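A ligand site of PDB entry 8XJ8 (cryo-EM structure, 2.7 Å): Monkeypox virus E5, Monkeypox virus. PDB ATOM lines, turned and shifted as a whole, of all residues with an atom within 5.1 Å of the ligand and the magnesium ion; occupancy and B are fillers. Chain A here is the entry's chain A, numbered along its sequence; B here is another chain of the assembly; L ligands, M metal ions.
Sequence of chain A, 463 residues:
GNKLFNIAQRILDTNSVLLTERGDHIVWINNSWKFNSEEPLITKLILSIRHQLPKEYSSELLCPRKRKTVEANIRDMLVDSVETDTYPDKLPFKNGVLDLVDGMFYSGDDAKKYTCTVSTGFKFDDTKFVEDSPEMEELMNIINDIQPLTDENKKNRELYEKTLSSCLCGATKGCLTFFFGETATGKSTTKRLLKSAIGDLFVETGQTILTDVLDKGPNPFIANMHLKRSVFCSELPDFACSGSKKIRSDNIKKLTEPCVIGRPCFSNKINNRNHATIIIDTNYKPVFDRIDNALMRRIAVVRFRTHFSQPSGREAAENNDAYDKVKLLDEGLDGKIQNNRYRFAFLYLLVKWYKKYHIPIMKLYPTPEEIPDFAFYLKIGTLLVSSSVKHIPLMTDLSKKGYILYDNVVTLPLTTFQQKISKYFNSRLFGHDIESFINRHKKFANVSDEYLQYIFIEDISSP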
ATOM      1  N   ASN A 141     -30.388   6.121 -11.558  1.00  0.00           N
ATOM      2  CA  ASN A 141     -30.587   5.607 -10.204  1.00  0.00           C
ATOM      3  C   ASN A 141     -30.147   4.153 -10.108  1.00  0.00           C
ATOM      4  O   ASN A 141     -29.483   3.763  -9.137  1.00  0.00           O
ATOM      5  CB  ASN A 141     -32.061   5.756  -9.803  1.00  0.00           C
ATOM      6  CG  ASN A 141     -32.352   7.101  -9.183  1.00  0.00           C
ATOM      7  OD1 ASN A 141     -31.459   7.768  -8.659  1.00  0.00           O
ATOM      8  ND2 ASN A 141     -33.614   7.504  -9.210  1.00  0.00           N
ATOM      9  N   ILE A 142     -30.494   3.336 -11.103  1.00  0.00           N
ATOM     10  CA  ILE A 142     -30.124   1.926 -11.083  1.00  0.00           C
ATOM     11  C   ILE A 142     -28.610   1.768 -11.118  1.00  0.00           C
ATOM     12  O   ILE A 142     -28.022   0.986 -10.343  1.00  0.00           O
ATOM     13  CB  ILE A 142     -30.785   1.183 -12.256  1.00  0.00           C
ATOM     14  CG1 ILE A 142     -32.295   1.059 -12.026  1.00  0.00           C
ATOM     15  CG2 ILE A 142     -30.172  -0.191 -12.449  1.00  0.00           C
ATOM     16  CD1 ILE A 142     -33.088   0.895 -13.293  1.00  0.00           C
ATOM     17  N   ASP A 145     -27.049   2.723  -7.910  1.00  0.00           N
ATOM     18  CA  ASP A 145     -27.243   1.651  -6.941  1.00  0.00           C
ATOM     19  C   ASP A 145     -26.237   0.525  -7.138  1.00  0.00           C
ATOM     20  O   ASP A 145     -25.677   0.018  -6.165  1.00  0.00           O
ATOM     21  CB  ASP A 145     -28.673   1.109  -7.041  1.00  0.00           C
ATOM     22  CG  ASP A 145     -29.699   2.083  -6.519  1.00  0.00           C
ATOM     23  OD1 ASP A 145     -29.360   2.906  -5.636  1.00  0.00           O
ATOM     24  OD2 ASP A 145     -30.855   2.038  -6.993  1.00  0.00           O
ATOM     25  N   ILE A 146     -26.006   0.116  -8.383  1.00  0.00           N
ATOM     26  CA  ILE A 146     -25.089  -0.986  -8.642  1.00  0.00           C
ATOM     27  C   ILE A 146     -23.659  -0.599  -8.285  1.00  0.00           C
ATOM     28  O   ILE A 146     -22.946  -1.354  -7.609  1.00  0.00           O
ATOM     29  CB  ILE A 146     -25.208  -1.469 -10.103  1.00  0.00           C
ATOM     30  CG1 ILE A 146     -26.554  -2.138 -10.338  1.00  0.00           C
ATOM     31  CG2 ILE A 146     -24.073  -2.418 -10.447  1.00  0.00           C
ATOM     32  CD1 ILE A 146     -26.820  -2.477 -11.788  1.00  0.00           C
ATOM     33  N   GLY A 181     -18.152 -10.983  -8.050  1.00  0.00           N
ATOM     34  CA  GLY A 181     -18.960 -10.525  -6.928  1.00  0.00           C
ATOM     35  C   GLY A 181     -19.709 -11.663  -6.281  1.00  0.00           C
ATOM     36  O   GLY A 181     -19.748 -12.787  -6.784  1.00  0.00           O
ATOM     37  N   GLU A 182     -20.307 -11.352  -5.134  1.00  0.00           N
ATOM     38  CA  GLU A 182     -21.165 -12.278  -4.419  1.00  0.00           C
ATOM     39  C   GLU A 182     -22.550 -12.282  -5.069  1.00  0.00           C
ATOM     40  O   GLU A 182     -22.827 -11.545  -6.021  1.00  0.00           O
ATOM     41  CB  GLU A 182     -21.217 -11.900  -2.939  1.00  0.00           C
ATOM     42  CG  GLU A 182     -21.590 -13.047  -2.009  1.00  0.00           C
ATOM     43  CD  GLU A 182     -20.747 -14.283  -2.228  1.00  0.00           C
ATOM     44  OE1 GLU A 182     -19.524 -14.229  -1.979  1.00  0.00           O
ATOM     45  OE2 GLU A 182     -21.310 -15.317  -2.641  1.00  0.00           O
ATOM     46  N   THR A 183     -23.439 -13.139  -4.557  1.00  0.00           N
ATOM     47  CA  THR A 183     -24.743 -13.315  -5.169  1.00  0.00           C
ATOM     48  C   THR A 183     -25.604 -12.062  -5.015  1.00  0.00           C
ATOM     49  O   THR A 183     -25.485 -11.321  -4.036  1.00  0.00           O
ATOM     50  CB  THR A 183     -25.452 -14.528  -4.575  1.00  0.00           C
ATOM     51  OG1 THR A 183     -26.646 -14.801  -5.310  1.00  0.00           O
ATOM     52  CG2 THR A 183     -25.798 -14.299  -3.107  1.00  0.00           C
ATOM     53  N   ALA A 184     -26.460 -11.834  -6.010  1.00  0.00           N
ATOM     54  CA  ALA A 184     -27.410 -10.721  -6.016  1.00  0.00           C
ATOM     55  C   ALA A 184     -26.709  -9.378  -5.855  1.00  0.00           C
ATOM     56  O   ALA A 184     -27.040  -8.572  -4.983  1.00  0.00           O
ATOM     57  CB  ALA A 184     -28.488 -10.907  -4.941  1.00  0.00           C
ATOM     58  N   THR A 185     -25.737  -9.118  -6.729  1.00  0.00           N
ATOM     59  CA  THR A 185     -24.978  -7.876  -6.696  1.00  0.00           C
ATOM     60  C   THR A 185     -25.119  -7.047  -7.969  1.00  0.00           C
ATOM     61  O   THR A 185     -24.481  -5.991  -8.076  1.00  0.00           O
ATOM     62  CB  THR A 185     -23.500  -8.151  -6.424  1.00  0.00           C
ATOM     63  OG1 THR A 185     -23.060  -9.255  -7.224  1.00  0.00           O
ATOM     64  CG2 THR A 185     -23.272  -8.458  -4.956  1.00  0.00           C
ATOM     65  N   GLY A 186     -25.927  -7.485  -8.926  1.00  0.00           N
ATOM     66  CA  GLY A 186     -26.171  -6.715 -10.133  1.00  0.00           C
ATOM     67  C   GLY A 186     -25.303  -7.056 -11.315  1.00  0.00           C
ATOM     68  O   GLY A 186     -25.300  -6.292 -12.295  1.00  0.00           O
ATOM     69  N   LYS A 187     -24.561  -8.166 -11.274  1.00  0.00           N
ATOM     70  CA  LYS A 187     -23.682  -8.501 -12.390  1.00  0.00           C
ATOM     71  C   LYS A 187     -24.456  -8.940 -13.629  1.00  0.00           C
ATOM     72  O   LYS A 187     -24.010  -8.687 -14.746  1.00  0.00           O
ATOM     73  CB  LYS A 187     -22.706  -9.603 -11.965  1.00  0.00           C
ATOM     74  CG  LYS A 187     -22.013  -9.346 -10.633  1.00  0.00           C
ATOM     75  CD  LYS A 187     -20.984 -10.417 -10.334  1.00  0.00           C
ATOM     76  CE  LYS A 187     -21.621 -11.785 -10.145  1.00  0.00           C
ATOM     77  NZ  LYS A 187     -22.449 -11.842  -8.907  1.00  0.00           N
ATOM     78  N   SER A 188     -25.607  -9.588 -13.448  1.00  0.00           N
ATOM     79  CA  SER A 188     -26.423  -9.983 -14.595  1.00  0.00           C
ATOM     80  C   SER A 188     -27.272  -8.839 -15.118  1.00  0.00           C
ATOM     81  O   SER A 188     -27.610  -8.799 -16.304  1.00  0.00           O
ATOM     82  CB  SER A 188     -27.301 -11.175 -14.235  1.00  0.00           C
ATOM     83  OG  SER A 188     -26.523 -12.340 -14.008  1.00  0.00           O
ATOM     84  N   THR A 189     -27.635  -7.889 -14.239  1.00  0.00           N
ATOM     85  CA  THR A 189     -28.391  -6.722 -14.673  1.00  0.00           C
ATOM     86  C   THR A 189     -27.575  -5.890 -15.662  1.00  0.00           C
ATOM     87  O   THR A 189     -28.116  -5.407 -16.664  1.00  0.00           O
ATOM     88  CB  THR A 189     -28.796  -5.883 -13.463  1.00  0.00           C
ATOM     89  OG1 THR A 189     -29.439  -6.726 -12.501  1.00  0.00           O
ATOM     90  CG2 THR A 189     -29.752  -4.779 -13.880  1.00  0.00           C
ATOM     91  N   ARG A 192     -27.545  -7.717 -19.008  1.00  0.00           N
ATOM     92  CA  ARG A 192     -28.804  -7.574 -19.719  1.00  0.00           C
ATOM     93  C   ARG A 192     -28.963  -6.173 -20.298  1.00  0.00           C
ATOM     94  O   ARG A 192     -29.450  -6.007 -21.416  1.00  0.00           O
ATOM     95  CB  ARG A 192     -29.966  -7.903 -18.781  1.00  0.00           C
ATOM     96  CG  ARG A 192     -30.071  -9.380 -18.437  1.00  0.00           C
ATOM     97  CD  ARG A 192     -31.302  -9.665 -17.591  1.00  0.00           C
ATOM     98  NE  ARG A 192     -30.948 -10.179 -16.270  1.00  0.00           N
ATOM     99  CZ  ARG A 192     -31.207  -9.543 -15.134  1.00  0.00           C
ATOM    100  NH1 ARG A 192     -31.821  -8.371 -15.113  1.00  0.00           N
ATOM    101  NH2 ARG A 192     -30.850 -10.106 -13.985  1.00  0.00           N
ATOM    102  N   GLU A 235     -20.612 -17.468 -15.412  1.00  0.00           N
ATOM    103  CA  GLU A 235     -20.347 -18.504 -14.421  1.00  0.00           C
ATOM    104  C   GLU A 235     -18.963 -19.110 -14.563  1.00  0.00           C
ATOM    105  O   GLU A 235     -18.453 -19.284 -15.675  1.00  0.00           O
ATOM    106  CB  GLU A 235     -21.417 -19.608 -14.491  1.00  0.00           C
ATOM    107  CG  GLU A 235     -22.447 -19.516 -13.395  1.00  0.00           C
ATOM    108  CD  GLU A 235     -23.518 -18.480 -13.690  1.00  0.00           C
ATOM    109  OE1 GLU A 235     -23.792 -17.642 -12.808  1.00  0.00           O
ATOM    110  OE2 GLU A 235     -24.084 -18.509 -14.798  1.00  0.00           O
ATOM    111  N   ASP A 281     -18.507 -13.337 -15.971  1.00  0.00           N
ATOM    112  CA  ASP A 281     -19.263 -13.155 -14.735  1.00  0.00           C
ATOM    113  C   ASP A 281     -18.881 -14.251 -13.740  1.00  0.00           C
ATOM    114  O   ASP A 281     -18.988 -15.438 -14.052  1.00  0.00           O
ATOM    115  CB  ASP A 281     -20.754 -13.202 -15.022  1.00  0.00           C
ATOM    116  CG  ASP A 281     -21.415 -11.853 -14.860  1.00  0.00           C
ATOM    117  OD1 ASP A 281     -20.844 -10.994 -14.162  1.00  0.00           O
ATOM    118  OD2 ASP A 281     -22.504 -11.648 -15.435  1.00  0.00           O
ATOM    119  N   ASN A 283     -18.562 -15.627  -9.432  1.00  0.00           N
ATOM    120  CA  ASN A 283     -18.575 -15.609  -7.975  1.00  0.00           C
ATOM    121  C   ASN A 283     -17.238 -16.032  -7.380  1.00  0.00           C
ATOM    122  O   ASN A 283     -17.054 -15.936  -6.162  1.00  0.00           O
ATOM    123  CB  ASN A 283     -19.674 -16.528  -7.434  1.00  0.00           C
ATOM    124  CG  ASN A 283     -21.069 -16.026  -7.756  1.00  0.00           C
ATOM    125  OD1 ASN A 283     -21.684 -16.451  -8.724  1.00  0.00           O
ATOM    126  ND2 ASN A 283     -21.569 -15.115  -6.937  1.00  0.00           N
ATOM    127  N   PHE A 308     -28.881  -6.614  -3.284  1.00  0.00           N
ATOM    128  CA  PHE A 308     -30.297  -6.351  -3.492  1.00  0.00           C
ATOM    129  C   PHE A 308     -31.053  -7.544  -2.931  1.00  0.00           C
ATOM    130  O   PHE A 308     -31.050  -8.625  -3.513  1.00  0.00           O
ATOM    131  CB  PHE A 308     -30.602  -6.121  -4.974  1.00  0.00           C
ATOM    132  CG  PHE A 308     -29.703  -5.101  -5.613  1.00  0.00           C
ATOM    133  CD1 PHE A 308     -29.771  -3.767  -5.258  1.00  0.00           C
ATOM    134  CD2 PHE A 308     -28.776  -5.491  -6.569  1.00  0.00           C
ATOM    135  CE1 PHE A 308     -28.940  -2.841  -5.836  1.00  0.00           C
ATOM    136  CE2 PHE A 308     -27.939  -4.558  -7.151  1.00  0.00           C
ATOM    137  CZ  PHE A 308     -28.027  -3.235  -6.794  1.00  0.00           C
ATOM    138  N   LYS A 327     -29.700  -2.993  -0.271  1.00  0.00           N
ATOM    139  CA  LYS A 327     -30.853  -2.286  -0.810  1.00  0.00           C
ATOM    140  C   LYS A 327     -31.990  -3.273  -1.043  1.00  0.00           C
ATOM    141  O   LYS A 327     -31.811  -4.487  -0.932  1.00  0.00           O
ATOM    142  CB  LYS A 327     -30.490  -1.543  -2.105  1.00  0.00           C
ATOM    143  CG  LYS A 327     -31.375  -0.342  -2.400  1.00  0.00           C
ATOM    144  CD  LYS A 327     -31.042   0.281  -3.731  1.00  0.00           C
ATOM    145  CE  LYS A 327     -32.039   1.386  -4.070  1.00  0.00           C
ATOM    146  NZ  LYS A 327     -33.387   0.827  -4.390  1.00  0.00           N
ATOM    147  N   LEU A 328     -33.160  -2.743  -1.377  1.00  0.00           N
ATOM    148  CA  LEU A 328     -34.355  -3.547  -1.580  1.00  0.00           C
ATOM    149  C   LEU A 328     -34.438  -4.032  -3.020  1.00  0.00           C
ATOM    150  O   LEU A 328     -34.174  -3.261  -3.951  1.00  0.00           O
ATOM    151  CB  LEU A 328     -35.607  -2.750  -1.215  1.00  0.00           C
ATOM    152  CG  LEU A 328     -36.892  -3.556  -0.997  1.00  0.00           C
ATOM    153  CD1 LEU A 328     -36.670  -4.671   0.001  1.00  0.00           C
ATOM    154  CD2 LEU A 328     -38.020  -2.635  -0.532  1.00  0.00           C
ATOM    155  N   LEU A 329     -34.802  -5.297  -3.193  1.00  0.00           N
ATOM    156  CA  LEU A 329     -34.922  -5.858  -4.526  1.00  0.00           C
ATOM    157  C   LEU A 329     -36.184  -5.346  -5.222  1.00  0.00           C
ATOM    158  O   LEU A 329     -37.234  -5.188  -4.601  1.00  0.00           O
ATOM    159  CB  LEU A 329     -34.957  -7.388  -4.447  1.00  0.00           C
ATOM    160  CG  LEU A 329     -34.577  -8.182  -5.691  1.00  0.00           C
ATOM    161  CD1 LEU A 329     -33.885  -9.477  -5.303  1.00  0.00           C
ATOM    162  CD2 LEU A 329     -35.806  -8.480  -6.548  1.00  0.00           C
ATOM    163  N   ASP A 330     -36.062  -5.096  -6.529  1.00  0.00           N
ATOM    164  CA  ASP A 330     -37.185  -4.700  -7.357  1.00  0.00           C
ATOM    165  C   ASP A 330     -37.501  -5.831  -8.319  1.00  0.00           C
ATOM    166  O   ASP A 330     -36.654  -6.195  -9.149  1.00  0.00           O
ATOM    167  CB  ASP A 330     -36.873  -3.411  -8.127  1.00  0.00           C
ATOM    168  CG  ASP A 330     -38.117  -2.719  -8.631  1.00  0.00           C
ATOM    169  OD1 ASP A 330     -39.210  -2.985  -8.100  1.00  0.00           O
ATOM    170  OD2 ASP A 330     -37.996  -1.896  -9.570  1.00  0.00           O
ATOM    171  N   LEU A 333     -38.087  -4.876 -12.375  1.00  0.00           N
ATOM    172  CA  LEU A 333     -36.996  -4.363 -13.192  1.00  0.00           C
ATOM    173  C   LEU A 333     -36.588  -5.360 -14.273  1.00  0.00           C
ATOM    174  O   LEU A 333     -36.269  -4.965 -15.401  1.00  0.00           O
ATOM    175  CB  LEU A 333     -35.800  -4.026 -12.301  1.00  0.00           C
ATOM    176  CG  LEU A 333     -34.539  -3.517 -12.987  1.00  0.00           C
ATOM    177  CD1 LEU A 333     -34.842  -2.292 -13.829  1.00  0.00           C
ATOM    178  CD2 LEU A 333     -33.462  -3.199 -11.954  1.00  0.00           C
ATOM    179  N   ASP A 334     -36.586  -6.654 -13.945  1.00  0.00           N
ATOM    180  CA  ASP A 334     -36.176  -7.663 -14.910  1.00  0.00           C
ATOM    181  C   ASP A 334     -37.074  -7.657 -16.142  1.00  0.00           C
ATOM    182  O   ASP A 334     -36.595  -7.772 -17.277  1.00  0.00           O
ATOM    183  CB  ASP A 334     -36.163  -9.043 -14.254  1.00  0.00           C
ATOM    184  CG  ASP A 334     -34.862  -9.777 -14.468  1.00  0.00           C
ATOM    185  OD1 ASP A 334     -34.225  -9.562 -15.519  1.00  0.00           O
ATOM    186  OD2 ASP A 334     -34.483 -10.586 -13.592  1.00  0.00           O
ATOM    187  N   GLU B 257     -30.302 -19.207 -16.298  1.00  0.00           N
ATOM    188  CA  GLU B 257     -30.093 -18.023 -17.111  1.00  0.00           C
ATOM    189  C   GLU B 257     -31.108 -17.973 -18.261  1.00  0.00           C
ATOM    190  O   GLU B 257     -31.615 -19.009 -18.691  1.00  0.00           O
ATOM    191  CB  GLU B 257     -28.672 -18.008 -17.675  1.00  0.00           C
ATOM    192  CG  GLU B 257     -27.597 -17.902 -16.618  1.00  0.00           C
ATOM    193  CD  GLU B 257     -27.920 -16.885 -15.548  1.00  0.00           C
ATOM    194  OE1 GLU B 257     -27.946 -15.681 -15.863  1.00  0.00           O
ATOM    195  OE2 GLU B 257     -28.142 -17.288 -14.392  1.00  0.00           O
ATOM    196  N   ALA B 294     -24.931 -18.477  -3.678  1.00  0.00           N
ATOM    197  CA  ALA B 294     -25.571 -18.398  -4.991  1.00  0.00           C
ATOM    198  C   ALA B 294     -26.331 -19.669  -5.322  1.00  0.00           C
ATOM    199  O   ALA B 294     -27.342 -19.619  -6.034  1.00  0.00           O
ATOM    200  CB  ALA B 294     -24.522 -18.106  -6.062  1.00  0.00           C
ATOM    201  N   ARG B 297     -29.883 -19.981  -3.420  1.00  0.00           N
ATOM    202  CA  ARG B 297     -30.972 -19.147  -3.914  1.00  0.00           C
ATOM    203  C   ARG B 297     -31.704 -19.758  -5.102  1.00  0.00           C
ATOM    204  O   ARG B 297     -32.661 -19.147  -5.585  1.00  0.00           O
ATOM    205  CB  ARG B 297     -30.437 -17.766  -4.306  1.00  0.00           C
ATOM    206  CG  ARG B 297     -30.258 -16.809  -3.140  1.00  0.00           C
ATOM    207  CD  ARG B 297     -30.019 -15.382  -3.617  1.00  0.00           C
ATOM    208  NE  ARG B 297     -29.476 -15.343  -4.972  1.00  0.00           N
ATOM    209  CZ  ARG B 297     -30.045 -14.679  -5.975  1.00  0.00           C
ATOM    210  NH1 ARG B 297     -31.166 -14.012  -5.814  1.00  0.00           N
ATOM    211  NH2 ARG B 297     -29.458 -14.708  -7.172  1.00  0.00           N
ATOM    212  N   ARG B 298     -31.282 -20.926  -5.583  1.00  0.00           N
ATOM    213  CA  ARG B 298     -31.839 -21.513  -6.789  1.00  0.00           C
ATOM    214  C   ARG B 298     -32.430 -22.902  -6.567  1.00  0.00           C
ATOM    215  O   ARG B 298     -32.715 -23.595  -7.546  1.00  0.00           O
ATOM    216  CB  ARG B 298     -30.764 -21.585  -7.885  1.00  0.00           C
ATOM    217  CG  ARG B 298     -30.258 -20.233  -8.376  1.00  0.00           C
ATOM    218  CD  ARG B 298     -29.063 -20.427  -9.292  1.00  0.00           C
ATOM    219  NE  ARG B 298     -28.755 -19.237 -10.075  1.00  0.00           N
ATOM    220  CZ  ARG B 298     -28.103 -18.175  -9.614  1.00  0.00           C
ATOM    221  NH1 ARG B 298     -27.688 -18.115  -8.359  1.00  0.00           N
ATOM    222  NH2 ARG B 298     -27.865 -17.151 -10.419  1.00  0.00           N
HETATM  223  P1  LIG L   1     -25.787 -13.995  -8.832  1.00  0.00           P
HETATM  224  O1  LIG L   1     -26.241 -14.983  -7.806  1.00  0.00           O
HETATM  225  O2  LIG L   1     -24.370 -13.450  -8.441  1.00  0.00           O
HETATM  226  O3  LIG L   1     -25.693 -14.715 -10.239  1.00  0.00           O
HETATM  227  P2  LIG L   1     -26.233 -11.429  -9.754  1.00  0.00           P
HETATM  228  O4  LIG L   1     -24.868 -11.147  -9.237  1.00  0.00           O
HETATM  229  O5  LIG L   1     -26.135 -11.778 -11.261  1.00  0.00           O
HETATM  230  N1  LIG L   1     -26.895 -12.725  -8.933  1.00  0.00           N
HETATM  231  P3  LIG L   1     -28.553 -10.049 -10.248  1.00  0.00           P
HETATM  232  O6  LIG L   1     -29.205 -11.368 -10.378  1.00  0.00           O
HETATM  233  O7  LIG L   1     -28.370  -9.329 -11.595  1.00  0.00           O
HETATM  234  O8  LIG L   1     -27.121 -10.151  -9.578  1.00  0.00           O
HETATM  235  O9  LIG L   1     -29.422  -9.159  -9.271  1.00  0.00           O
HETATM  236  C1  LIG L   1     -30.243  -9.740  -8.241  1.00  0.00           C
HETATM  237  C2  LIG L   1     -31.622  -9.129  -8.301  1.00  0.00           C
HETATM  238  O10 LIG L   1     -31.536  -7.721  -7.987  1.00  0.00           O
HETATM  239  C3  LIG L   1     -32.339  -9.235  -9.648  1.00  0.00           C
HETATM  240  O11 LIG L   1     -33.681  -9.663  -9.473  1.00  0.00           O
HETATM  241  C4  LIG L   1     -32.257  -7.818 -10.215  1.00  0.00           C
HETATM  242  O12 LIG L   1     -33.372  -7.511 -11.048  1.00  0.00           O
HETATM  243  C5  LIG L   1     -32.279  -6.984  -8.942  1.00  0.00           C
HETATM  244  N2  LIG L   1     -31.679  -5.664  -9.074  1.00  0.00           N
HETATM  245  C6  LIG L   1     -30.520  -5.353  -9.741  1.00  0.00           C
HETATM  246  N3  LIG L   1     -30.214  -4.077  -9.713  1.00  0.00           N
HETATM  247  C7  LIG L   1     -31.245  -3.508  -8.966  1.00  0.00           C
HETATM  248  C8  LIG L   1     -31.504  -2.183  -8.571  1.00  0.00           C
HETATM  249  N4  LIG L   1     -30.725  -1.151  -8.873  1.00  0.00           N
HETATM  250  N5  LIG L   1     -32.627  -1.963  -7.849  1.00  0.00           N
HETATM  251  C9  LIG L   1     -33.415  -2.994  -7.536  1.00  0.00           C
HETATM  252  N6  LIG L   1     -33.269  -4.282  -7.855  1.00  0.00           N
HETATM  253  C10 LIG L   1     -32.154  -4.479  -8.576  1.00  0.00           C
HETATM  254 MG    MG M   1     -26.033 -13.565 -12.380  1.00  0.00          MG
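O7 of the ligand lies within hydrogen-bond range of N of Ser 188 (3.3 Å).
OG1 of Thr 183 sits at hydrogen-bond distance from O1 of the ligand (2.5 Å).
NZ of Lys 187 is in salt-bridge range of O4 of the ligand (2.5 Å).
N of Thr 189 lies within hydrogen-bond range of O7 of the ligand, at 3.1 Å.
O7 of the ligand sits at hydrogen-bond distance from OG1 of Thr 189.
The backbone NH (N) of Gly 186 lies within hydrogen-bond range of an oxygen (O8) of the ligand, 3.0 Å away.
The backbone NH (N) of Asp 330 is in hydrogen-bond range of a nitrogen (N6) of the ligand (3.2 Å).
The guanidinium group (NH1) of Arg 298 of chain B lies within salt-bridge range of an oxygen (O1) of the ligand, 3.5 Å away.
The guanidinium group (NH2) of Arg 297 of chain B is in salt-bridge range of an oxygen (O1) of the ligand (3.3 Å).
The backbone NH (N) of Thr 185 lies within hydrogen-bond range of an oxygen (O8) of the ligand.
The side-chain hydroxyl (OG1) of Thr 185 is in hydrogen-bond range of an oxygen (O4) of the ligand (3.3 Å).
The guanidinium group (NH2) of Arg 192 lies within salt-bridge range of an oxygen (O7) of the ligand, 3.5 Å away.
OG of Ser 188 is bound to the magnesium ion, 2.1 Å away.
An oxygen (O5) of the ligand binds the magnesium ion (2.1 Å).
O3 of the ligand is bound to the magnesium ion, 2.5 Å away.
The magnesium ion has three donor atoms within binding distance.
The side-chain hydroxyl of Thr 183 is in hydrogen-bond range of the guanidinium group of Arg 297 of chain B (2.9 Å).
NZ of Lys 187 sits at hydrogen-bond distance from O of Glu 182, 2.9 Å away.
O of Ala 184 lies within hydrogen-bond range of N of Phe 308 (3.2 Å).
NH2 of Arg 298 of chain B lies within salt-bridge range of OE2 of Glu 257 of chain B (3.99 Å).
OG1 of Thr 185 is in hydrogen-bond range of O of Glu 182 (2.6 Å).
The side-chain carboxylate (OD1) of Asp 334 is in salt-bridge range of the guanidinium group (NH1) of Arg 192, 2.7 Å away.
OD2 of Asp 145 is in salt-bridge range of NZ of Lys 327, 3.8 Å away.
ND2 of Asn 283 is in hydrogen-bond range of O of Gly 181 (3.0 Å).
O of Glu 182 lies close to O2 of the ligand.
The backbone NH (N) of Ala 184 sits close to a nitrogen (N1) of the ligand (3.1 Å).
Merely in contact with the ligand: Phe 308, Asp 145, Asn 283, Leu 328, Leu 333, Ile 142, Leu 329 and Ala 294 of chain B.
Of the 28 residues printed, 1 comes within 4 Å of the magnesium ion.
The nearest printed residue that does not touch the magnesium ion is Arg 298 of chain B (4.5 Å).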
